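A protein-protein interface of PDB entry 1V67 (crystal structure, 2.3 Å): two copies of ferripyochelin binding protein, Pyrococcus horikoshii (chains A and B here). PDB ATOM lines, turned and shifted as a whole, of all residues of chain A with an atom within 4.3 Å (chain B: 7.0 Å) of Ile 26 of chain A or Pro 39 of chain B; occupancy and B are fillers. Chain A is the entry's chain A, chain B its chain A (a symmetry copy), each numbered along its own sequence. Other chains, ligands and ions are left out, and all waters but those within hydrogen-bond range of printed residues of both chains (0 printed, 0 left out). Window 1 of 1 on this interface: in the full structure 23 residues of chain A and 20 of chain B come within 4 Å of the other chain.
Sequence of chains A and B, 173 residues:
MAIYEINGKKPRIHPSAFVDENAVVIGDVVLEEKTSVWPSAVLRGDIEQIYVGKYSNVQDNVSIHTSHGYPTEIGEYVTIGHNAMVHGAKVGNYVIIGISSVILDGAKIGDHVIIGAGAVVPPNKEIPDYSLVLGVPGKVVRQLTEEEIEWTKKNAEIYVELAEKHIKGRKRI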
ATOM      1  N   TYR A   4      25.106  -6.861  32.732  1.00  0.00           N
ATOM      2  CA  TYR A   4      25.042  -6.031  31.534  1.00  0.00           C
ATOM      3  C   TYR A   4      23.588  -5.887  31.124  1.00  0.00           C
ATOM      4  O   TYR A   4      22.722  -6.651  31.543  1.00  0.00           O
ATOM      5  CB  TYR A   4      25.802  -6.685  30.368  1.00  0.00           C
ATOM      6  CG  TYR A   4      27.238  -7.042  30.655  1.00  0.00           C
ATOM      7  CD1 TYR A   4      28.284  -6.208  30.250  1.00  0.00           C
ATOM      8  CD2 TYR A   4      27.549  -8.215  31.337  1.00  0.00           C
ATOM      9  CE1 TYR A   4      29.617  -6.542  30.516  1.00  0.00           C
ATOM     10  CE2 TYR A   4      28.874  -8.559  31.613  1.00  0.00           C
ATOM     11  CZ  TYR A   4      29.901  -7.721  31.202  1.00  0.00           C
ATOM     12  OH  TYR A   4      31.202  -8.071  31.483  1.00  0.00           O
ATOM     13  N   VAL A  24      27.560 -14.217  34.862  1.00  0.00           N
ATOM     14  CA  VAL A  24      27.257 -13.206  33.853  1.00  0.00           C
ATOM     15  C   VAL A  24      25.763 -13.173  33.545  1.00  0.00           C
ATOM     16  O   VAL A  24      25.160 -14.187  33.195  1.00  0.00           O
ATOM     17  CB  VAL A  24      28.056 -13.459  32.538  1.00  0.00           C
ATOM     18  CG1 VAL A  24      27.710 -12.409  31.482  1.00  0.00           C
ATOM     19  CG2 VAL A  24      29.552 -13.422  32.826  1.00  0.00           C
ATOM     20  N   VAL A  25      25.154 -12.009  33.725  1.00  0.00           N
ATOM     21  CA  VAL A  25      23.731 -11.836  33.440  1.00  0.00           C
ATOM     22  C   VAL A  25      23.617 -10.784  32.354  1.00  0.00           C
ATOM     23  O   VAL A  25      24.102  -9.664  32.511  1.00  0.00           O
ATOM     24  CB  VAL A  25      22.998 -11.348  34.674  1.00  0.00           C
ATOM     25  CG1 VAL A  25      21.510 -11.214  34.379  1.00  0.00           C
ATOM     26  CG2 VAL A  25      23.244 -12.324  35.816  1.00  0.00           C
ATOM     27  N   ILE A  26      22.977 -11.138  31.252  1.00  0.00           N
ATOM     28  CA  ILE A  26      22.858 -10.203  30.164  1.00  0.00           C
ATOM     29  C   ILE A  26      21.414  -9.995  29.716  1.00  0.00           C
ATOM     30  O   ILE A  26      20.651 -10.944  29.588  1.00  0.00           O
ATOM     31  CB  ILE A  26      23.671 -10.695  28.954  1.00  0.00           C
ATOM     32  CG1 ILE A  26      25.169 -10.763  29.292  1.00  0.00           C
ATOM     33  CG2 ILE A  26      23.423  -9.789  27.781  1.00  0.00           C
ATOM     34  CD1 ILE A  26      26.017 -11.289  28.150  1.00  0.00           C
ATOM     35  N   GLY A  27      21.057  -8.737  29.485  1.00  0.00           N
ATOM     36  CA  GLY A  27      19.738  -8.393  28.994  1.00  0.00           C
ATOM     37  C   GLY A  27      18.493  -8.749  29.778  1.00  0.00           C
ATOM     38  O   GLY A  27      18.483  -8.710  31.008  1.00  0.00           O
ATOM     39  N   ASP A  28      17.442  -9.095  29.033  1.00  0.00           N
ATOM     40  CA  ASP A  28      16.141  -9.440  29.579  1.00  0.00           C
ATOM     41  C   ASP A  28      16.211 -10.684  30.437  1.00  0.00           C
ATOM     42  O   ASP A  28      16.020 -11.807  29.957  1.00  0.00           O
ATOM     43  CB  ASP A  28      15.145  -9.646  28.440  1.00  0.00           C
ATOM     44  CG  ASP A  28      13.716  -9.770  28.921  1.00  0.00           C
ATOM     45  OD1 ASP A  28      13.452  -9.660  30.144  1.00  0.00           O
ATOM     46  OD2 ASP A  28      12.847  -9.983  28.052  1.00  0.00           O
ATOM     47  N   VAL A  29      16.498 -10.486  31.717  1.00  0.00           N
ATOM     48  CA  VAL A  29      16.585 -11.609  32.648  1.00  0.00           C
ATOM     49  C   VAL A  29      15.932 -11.209  33.956  1.00  0.00           C
ATOM     50  O   VAL A  29      16.226 -10.155  34.494  1.00  0.00           O
ATOM     51  CB  VAL A  29      18.055 -11.993  32.921  1.00  0.00           C
ATOM     52  CG1 VAL A  29      18.127 -13.226  33.816  1.00  0.00           C
ATOM     53  CG2 VAL A  29      18.751 -12.260  31.612  1.00  0.00           C
ATOM     54  N   VAL A  42      26.094 -18.518  33.461  1.00  0.00           N
ATOM     55  CA  VAL A  42      25.791 -17.538  32.425  1.00  0.00           C
ATOM     56  C   VAL A  42      24.307 -17.529  32.067  1.00  0.00           C
ATOM     57  O   VAL A  42      23.735 -18.555  31.699  1.00  0.00           O
ATOM     58  CB  VAL A  42      26.632 -17.803  31.138  1.00  0.00           C
ATOM     59  CG1 VAL A  42      26.204 -16.864  30.023  1.00  0.00           C
ATOM     60  CG2 VAL A  42      28.122 -17.602  31.438  1.00  0.00           C
ATOM     61  N   LEU A  43      23.680 -16.368  32.225  1.00  0.00           N
ATOM     62  CA  LEU A  43      22.268 -16.196  31.891  1.00  0.00           C
ATOM     63  C   LEU A  43      22.198 -15.133  30.799  1.00  0.00           C
ATOM     64  O   LEU A  43      22.102 -13.944  31.080  1.00  0.00           O
ATOM     65  CB  LEU A  43      21.467 -15.753  33.120  1.00  0.00           C
ATOM     66  CG  LEU A  43      21.292 -16.825  34.203  1.00  0.00           C
ATOM     67  CD1 LEU A  43      22.569 -16.949  35.017  1.00  0.00           C
ATOM     68  CD2 LEU A  43      20.142 -16.446  35.098  1.00  0.00           C
ATOM     69  N   ARG A  44      22.252 -15.581  29.553  1.00  0.00           N
ATOM     70  CA  ARG A  44      22.256 -14.682  28.419  1.00  0.00           C
ATOM     71  C   ARG A  44      20.861 -14.396  27.877  1.00  0.00           C
ATOM     72  O   ARG A  44      20.324 -15.156  27.073  1.00  0.00           O
ATOM     73  CB  ARG A  44      23.140 -15.268  27.309  1.00  0.00           C
ATOM     74  CG  ARG A  44      23.435 -14.328  26.136  1.00  0.00           C
ATOM     75  CD  ARG A  44      24.864 -14.532  25.597  1.00  0.00           C
ATOM     76  NE  ARG A  44      25.088 -15.895  25.116  1.00  0.00           N
ATOM     77  CZ  ARG A  44      24.751 -16.326  23.903  1.00  0.00           C
ATOM     78  NH1 ARG A  44      24.176 -15.502  23.032  1.00  0.00           N
ATOM     79  NH2 ARG A  44      24.979 -17.586  23.561  1.00  0.00           N
ATOM     80  N   GLY A  45      20.279 -13.279  28.293  1.00  0.00           N
ATOM     81  CA  GLY A  45      18.945 -12.941  27.826  1.00  0.00           C
ATOM     82  C   GLY A  45      18.995 -12.015  26.652  1.00  0.00           C
ATOM     83  O   GLY A  45      18.476 -10.906  26.705  1.00  0.00           O
ATOM     84  N   PHE B  18      33.925 -10.966  17.536  1.00  0.00           N
ATOM     85  CA  PHE B  18      33.414 -10.565  18.834  1.00  0.00           C
ATOM     86  C   PHE B  18      33.989 -11.508  19.892  1.00  0.00           C
ATOM     87  O   PHE B  18      33.974 -12.729  19.730  1.00  0.00           O
ATOM     88  CB  PHE B  18      31.878 -10.625  18.856  1.00  0.00           C
ATOM     89  CG  PHE B  18      31.294 -10.521  20.242  1.00  0.00           C
ATOM     90  CD1 PHE B  18      31.484  -9.372  21.005  1.00  0.00           C
ATOM     91  CD2 PHE B  18      30.576 -11.577  20.793  1.00  0.00           C
ATOM     92  CE1 PHE B  18      30.994  -9.289  22.308  1.00  0.00           C
ATOM     93  CE2 PHE B  18      30.083 -11.503  22.095  1.00  0.00           C
ATOM     94  CZ  PHE B  18      30.284 -10.353  22.850  1.00  0.00           C
ATOM     95  N   VAL B  19      34.514 -10.930  20.963  1.00  0.00           N
ATOM     96  CA  VAL B  19      35.083 -11.714  22.043  1.00  0.00           C
ATOM     97  C   VAL B  19      34.665 -11.106  23.367  1.00  0.00           C
ATOM     98  O   VAL B  19      35.185 -10.072  23.784  1.00  0.00           O
ATOM     99  CB  VAL B  19      36.626 -11.746  21.983  1.00  0.00           C
ATOM    100  CG1 VAL B  19      37.165 -12.700  23.044  1.00  0.00           C
ATOM    101  CG2 VAL B  19      37.090 -12.185  20.601  1.00  0.00           C
ATOM    102  N   ASP B  20      33.714 -11.760  24.020  1.00  0.00           N
ATOM    103  CA  ASP B  20      33.198 -11.316  25.307  1.00  0.00           C
ATOM    104  C   ASP B  20      34.349 -11.155  26.300  1.00  0.00           C
ATOM    105  O   ASP B  20      35.261 -11.976  26.330  1.00  0.00           O
ATOM    106  CB  ASP B  20      32.209 -12.354  25.834  1.00  0.00           C
ATOM    107  CG  ASP B  20      31.330 -11.808  26.920  1.00  0.00           C
ATOM    108  OD1 ASP B  20      30.304 -11.180  26.584  1.00  0.00           O
ATOM    109  OD2 ASP B  20      31.670 -11.990  28.107  1.00  0.00           O
ATOM    110  N   GLU B  21      34.301 -10.118  27.131  1.00  0.00           N
ATOM    111  CA  GLU B  21      35.378  -9.890  28.099  1.00  0.00           C
ATOM    112  C   GLU B  21      35.436 -10.949  29.198  1.00  0.00           C
ATOM    113  O   GLU B  21      36.415 -11.036  29.950  1.00  0.00           O
ATOM    114  CB  GLU B  21      35.262  -8.484  28.706  1.00  0.00           C
ATOM    115  CG  GLU B  21      33.869  -8.058  29.088  1.00  0.00           C
ATOM    116  CD  GLU B  21      33.872  -6.769  29.885  1.00  0.00           C
ATOM    117  OE1 GLU B  21      34.624  -5.838  29.518  1.00  0.00           O
ATOM    118  OE2 GLU B  21      33.120  -6.686  30.877  1.00  0.00           O
ATOM    119  N   ASN B  22      34.383 -11.765  29.261  1.00  0.00           N
ATOM    120  CA  ASN B  22      34.264 -12.842  30.243  1.00  0.00           C
ATOM    121  C   ASN B  22      34.761 -14.160  29.626  1.00  0.00           C
ATOM    122  O   ASN B  22      34.847 -15.186  30.302  1.00  0.00           O
ATOM    123  CB  ASN B  22      32.803 -12.972  30.730  1.00  0.00           C
ATOM    124  CG  ASN B  22      32.230 -11.654  31.263  1.00  0.00           C
ATOM    125  OD1 ASN B  22      31.266 -11.122  30.713  1.00  0.00           O
ATOM    126  ND2 ASN B  22      32.816 -11.134  32.336  1.00  0.00           N
ATOM    127  N   ALA B  23      35.069 -14.128  28.332  1.00  0.00           N
ATOM    128  CA  ALA B  23      35.605 -15.299  27.646  1.00  0.00           C
ATOM    129  C   ALA B  23      37.124 -15.224  27.848  1.00  0.00           C
ATOM    130  O   ALA B  23      37.638 -14.190  28.265  1.00  0.00           O
ATOM    131  CB  ALA B  23      35.247 -15.231  26.162  1.00  0.00           C
ATOM    132  N   VAL B  24      37.844 -16.306  27.583  1.00  0.00           N
ATOM    133  CA  VAL B  24      39.294 -16.274  27.745  1.00  0.00           C
ATOM    134  C   VAL B  24      39.993 -16.849  26.517  1.00  0.00           C
ATOM    135  O   VAL B  24      39.728 -17.976  26.100  1.00  0.00           O
ATOM    136  CB  VAL B  24      39.742 -17.058  29.016  1.00  0.00           C
ATOM    137  CG1 VAL B  24      41.263 -17.038  29.160  1.00  0.00           C
ATOM    138  CG2 VAL B  24      39.102 -16.443  30.256  1.00  0.00           C
ATOM    139  N   VAL B  37      33.099 -15.400  20.188  1.00  0.00           N
ATOM    140  CA  VAL B  37      33.434 -16.176  21.371  1.00  0.00           C
ATOM    141  C   VAL B  37      32.575 -15.555  22.457  1.00  0.00           C
ATOM    142  O   VAL B  37      32.713 -14.370  22.777  1.00  0.00           O
ATOM    143  CB  VAL B  37      34.886 -16.029  21.761  1.00  0.00           C
ATOM    144  CG1 VAL B  37      35.196 -17.009  22.883  1.00  0.00           C
ATOM    145  CG2 VAL B  37      35.776 -16.270  20.551  1.00  0.00           C
ATOM    146  N   TRP B  38      31.701 -16.370  23.033  1.00  0.00           N
ATOM    147  CA  TRP B  38      30.749 -15.893  24.019  1.00  0.00           C
ATOM    148  C   TRP B  38      31.119 -15.984  25.494  1.00  0.00           C
ATOM    149  O   TRP B  38      32.152 -16.552  25.845  1.00  0.00           O
ATOM    150  CB  TRP B  38      29.390 -16.549  23.726  1.00  0.00           C
ATOM    151  CG  TRP B  38      28.982 -16.307  22.293  1.00  0.00           C
ATOM    152  CD1 TRP B  38      29.362 -17.030  21.192  1.00  0.00           C
ATOM    153  CD2 TRP B  38      28.208 -15.209  21.800  1.00  0.00           C
ATOM    154  NE1 TRP B  38      28.859 -16.453  20.051  1.00  0.00           N
ATOM    155  CE2 TRP B  38      28.134 -15.345  20.399  1.00  0.00           C
ATOM    156  CE3 TRP B  38      27.526 -14.150  22.414  1.00  0.00           C
ATOM    157  CZ2 TRP B  38      27.458 -14.422  19.596  1.00  0.00           C
ATOM    158  CZ3 TRP B  38      26.851 -13.242  21.617  1.00  0.00           C
ATOM    159  CH2 TRP B  38      26.804 -13.395  20.228  1.00  0.00           C
ATOM    160  N   PRO B  39      30.273 -15.414  26.375  1.00  0.00           N
ATOM    161  CA  PRO B  39      30.538 -15.428  27.811  1.00  0.00           C
ATOM    162  C   PRO B  39      31.072 -16.737  28.403  1.00  0.00           C
ATOM    163  O   PRO B  39      30.502 -17.806  28.201  1.00  0.00           O
ATOM    164  CB  PRO B  39      29.197 -15.013  28.411  1.00  0.00           C
ATOM    165  CG  PRO B  39      28.667 -14.061  27.385  1.00  0.00           C
ATOM    166  CD  PRO B  39      28.949 -14.817  26.101  1.00  0.00           C
ATOM    167  N   SER B  40      32.184 -16.628  29.130  1.00  0.00           N
ATOM    168  CA  SER B  40      32.798 -17.767  29.826  1.00  0.00           C
ATOM    169  C   SER B  40      33.404 -18.912  29.005  1.00  0.00           C
ATOM    170  O   SER B  40      33.755 -19.965  29.549  1.00  0.00           O
ATOM    171  CB  SER B  40      31.771 -18.332  30.804  1.00  0.00           C
ATOM    172  OG  SER B  40      32.378 -19.132  31.803  1.00  0.00           O
ATOM    173  N   ALA B  41      33.523 -18.706  27.700  1.00  0.00           N
ATOM    174  CA  ALA B  41      34.102 -19.720  26.830  1.00  0.00           C
ATOM    175  C   ALA B  41      35.608 -19.647  27.042  1.00  0.00           C
ATOM    176  O   ALA B  41      36.124 -18.611  27.454  1.00  0.00           O
ATOM    177  CB  ALA B  41      33.756 -19.416  25.372  1.00  0.00           C
ATOM    178  N   VAL B  42      36.316 -20.735  26.770  1.00  0.00           N
ATOM    179  CA  VAL B  42      37.764 -20.743  26.943  1.00  0.00           C
ATOM    180  C   VAL B  42      38.477 -21.364  25.744  1.00  0.00           C
ATOM    181  O   VAL B  42      38.205 -22.502  25.363  1.00  0.00           O
ATOM    182  CB  VAL B  42      38.171 -21.507  28.240  1.00  0.00           C
ATOM    183  CG1 VAL B  42      39.682 -21.627  28.332  1.00  0.00           C
ATOM    184  CG2 VAL B  42      37.637 -20.766  29.472  1.00  0.00           C
ATOM    185  N   VAL B  58      31.540 -19.780  19.272  1.00  0.00           N
ATOM    186  CA  VAL B  58      31.910 -20.621  20.414  1.00  0.00           C
ATOM    187  C   VAL B  58      31.070 -20.110  21.593  1.00  0.00           C
ATOM    188  O   VAL B  58      31.373 -19.076  22.187  1.00  0.00           O
ATOM    189  CB  VAL B  58      33.415 -20.470  20.725  1.00  0.00           C
ATOM    190  CG1 VAL B  58      33.875 -21.536  21.734  1.00  0.00           C
ATOM    191  CG2 VAL B  58      34.201 -20.578  19.434  1.00  0.00           C
ATOM    192  N   GLN B  59      30.006 -20.838  21.909  1.00  0.00           N
ATOM    193  CA  GLN B  59      29.091 -20.435  22.969  1.00  0.00           C
ATOM    194  C   GLN B  59      29.624 -20.482  24.394  1.00  0.00           C
ATOM    195  O   GLN B  59      30.777 -20.820  24.611  1.00  0.00           O
ATOM    196  CB  GLN B  59      27.771 -21.202  22.810  1.00  0.00           C
ATOM    197  CG  GLN B  59      26.965 -20.653  21.601  1.00  0.00           C
ATOM    198  CD  GLN B  59      26.005 -21.645  20.974  1.00  0.00           C
ATOM    199  OE1 GLN B  59      25.298 -22.373  21.677  1.00  0.00           O
ATOM    200  NE2 GLN B  59      25.958 -21.666  19.640  1.00  0.00           N
ATOM    201  N   ASP B  60      28.776 -20.110  25.347  1.00  0.00           N
ATOM    202  CA  ASP B  60      29.105 -20.020  26.770  1.00  0.00           C
ATOM    203  C   ASP B  60      29.566 -21.310  27.454  1.00  0.00           C
ATOM    204  O   ASP B  60      29.071 -22.389  27.137  1.00  0.00           O
ATOM    205  CB  ASP B  60      27.880 -19.478  27.515  1.00  0.00           C
ATOM    206  CG  ASP B  60      27.106 -18.438  26.698  1.00  0.00           C
ATOM    207  OD1 ASP B  60      27.347 -17.221  26.877  1.00  0.00           O
ATOM    208  OD2 ASP B  60      26.265 -18.841  25.860  1.00  0.00           O
ATOM    209  N   ASN B  61      30.509 -21.165  28.393  1.00  0.00           N
ATOM    210  CA  ASN B  61      31.059 -22.265  29.188  1.00  0.00           C
ATOM    211  C   ASN B  61      31.595 -23.419  28.371  1.00  0.00           C
ATOM    212  O   ASN B  61      31.642 -24.575  28.818  1.00  0.00           O
ATOM    213  CB  ASN B  61      30.015 -22.771  30.191  1.00  0.00           C
ATOM    214  CG  ASN B  61      29.782 -21.796  31.324  1.00  0.00           C
ATOM    215  OD1 ASN B  61      30.725 -21.400  32.001  1.00  0.00           O
ATOM    216  ND2 ASN B  61      28.532 -21.413  31.543  1.00  0.00           N
ATOM    217  N   VAL B  62      32.001 -23.071  27.164  1.00  0.00           N
ATOM    218  CA  VAL B  62      32.571 -24.004  26.223  1.00  0.00           C
ATOM    219  C   VAL B  62      34.089 -23.977  26.421  1.00  0.00           C
ATOM    220  O   VAL B  62      34.656 -22.943  26.754  1.00  0.00           O
ATOM    221  CB  VAL B  62      32.265 -23.551  24.786  1.00  0.00           C
ATOM    222  CG1 VAL B  62      33.295 -24.125  23.827  1.00  0.00           C
ATOM    223  CG2 VAL B  62      30.870 -23.996  24.374  1.00  0.00           C
ATOM    224  N   HIS B 166      25.661  -7.437  20.224  1.00  0.00           N
ATOM    225  CA  HIS B 166      26.355  -7.217  21.490  1.00  0.00           C
ATOM    226  C   HIS B 166      27.452  -6.178  21.337  1.00  0.00           C
ATOM    227  O   HIS B 166      27.685  -5.374  22.237  1.00  0.00           O
ATOM    228  CB  HIS B 166      26.960  -8.528  22.006  1.00  0.00           C
ATOM    229  CG  HIS B 166      25.953  -9.470  22.587  1.00  0.00           C
ATOM    230  ND1 HIS B 166      25.871  -9.733  23.938  1.00  0.00           N
ATOM    231  CD2 HIS B 166      24.965 -10.188  22.005  1.00  0.00           C
ATOM    232  CE1 HIS B 166      24.877 -10.572  24.161  1.00  0.00           C
ATOM    233  NE2 HIS B 166      24.310 -10.864  23.006  1.00  0.00           N
ATOM    234  N   ARG B 170      25.562  -3.789  23.712  1.00  0.00           N
ATOM    235  CA  ARG B 170      25.890  -4.318  25.032  1.00  0.00           C
ATOM    236  C   ARG B 170      26.393  -3.180  25.903  1.00  0.00           C
ATOM    237  O   ARG B 170      27.112  -2.296  25.434  1.00  0.00           O
ATOM    238  CB  ARG B 170      26.963  -5.407  24.935  1.00  0.00           C
ATOM    239  CG  ARG B 170      26.416  -6.821  24.954  1.00  0.00           C
ATOM    240  CD  ARG B 170      26.060  -7.260  26.366  1.00  0.00           C
ATOM    241  NE  ARG B 170      27.235  -7.660  27.143  1.00  0.00           N
ATOM    242  CZ  ARG B 170      27.994  -8.722  26.873  1.00  0.00           C
ATOM    243  NH1 ARG B 170      27.714  -9.507  25.841  1.00  0.00           N
ATOM    244  NH2 ARG B 170      29.036  -9.004  27.641  1.00  0.00           N
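The side-chain hydroxyl (OH) of Tyr 4 of chain A sits at hydrogen-bond distance from the side-chain carboxylate (OE2) of Glu 21 of chain B (2.4 Å).
OD1 of Asn 22 of chain B lies within hydrogen-bond range of OH of Tyr 4 of chain A (3.1 Å).
The guanidinium group (NH2) of Arg 44 of chain A is in salt-bridge range of the side-chain carboxylate (OD2) of Asp 60 of chain B, 2.9 Å away.
The backbone NH of Leu 43 of chain A sits at hydrogen-bond distance from the backbone carbonyl oxygen of Val 24 of chain A.
O of Ile 26 of chain A sits at hydrogen-bond distance from N of Gly 45 of chain A (2.7 Å).
The side-chain carboxylate of Asp 20 of chain B sits close to the side-chain amide oxygen of Asn 22 of chain B, 2.8 Å away.
The guanidinium group of Arg 170 of chain B lies within salt-bridge range of the side-chain carboxylate of Asp 20 of chain B (2.7 Å).
The backbone carbonyl oxygen of Pro 39 of chain B sits at hydrogen-bond distance from the backbone NH of Asn 61 of chain B.
A ring nitrogen (ND1) of His 166 of chain B is in hydrogen-bond range of the guanidinium group of Arg 170 of chain B (2.7 Å).
Among the printed residues, pairs that only touch across the chains: Val 42 of chain A with Asp 60 of chain B, Ile 26 of chain A with Arg 170 of chain B, Val 24 of chain A with Asn 22 of chain B, Tyr 4 of chain A with Arg 170 of chain B, Arg 44 of chain A with Trp 38 of chain B, Val 42 of chain A with Ser 40 of chain B, Val 42 of chain A with Asn 61 of chain B, Val 42 of chain A with Pro 39 of chain B, Ile 26 of chain A with Pro 39 of chain B and Ile 26 of chain A with His 166 of chain B.
Of chain B, only Pro 39 (3.9 Å), His 166 (3.98 Å) and Arg 170 (3.4 Å) come within 4 Å of Ile 26 of chain A.
Printed residues of chain A within 4 Å of Glu 21 of chain B: Tyr 4.
Of the printed residues of chain A, Asn 22 of chain B touches Tyr 4 and Val 24.
Of the printed residues of chain A, Trp 38 of chain B touches Arg 44.
Of the printed residues of chain A, Pro 39 of chain B touches Ile 26 and Val 42.
Of the printed residues of chain A, Ser 40 of chain B touches Val 42.
Of the printed residues of chain A, Asn 61 of chain B touches Val 42 (3.8 Å).
The nearest residue of chain B that does not touch Ile 26 of chain A is Asp 20 of chain B (4.6 Å).
The nearest printed residue of chain A that does not touch His 166 of chain B is Arg 44 of chain A (4.2 Å).
Printed residues of chain B that touch a printed residue of chain A: Glu 21, Asn 22, Trp 38, Pro 39, Ser 40, Asp 60, Asn 61, His 166 and Arg 170.
Hydrophobic or aromatic side chains of chain A that line the printed part of chain B: Tyr 4, Val 24, Ile 26 and Val 42.
Positions printed for both chains: 24 and 42.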
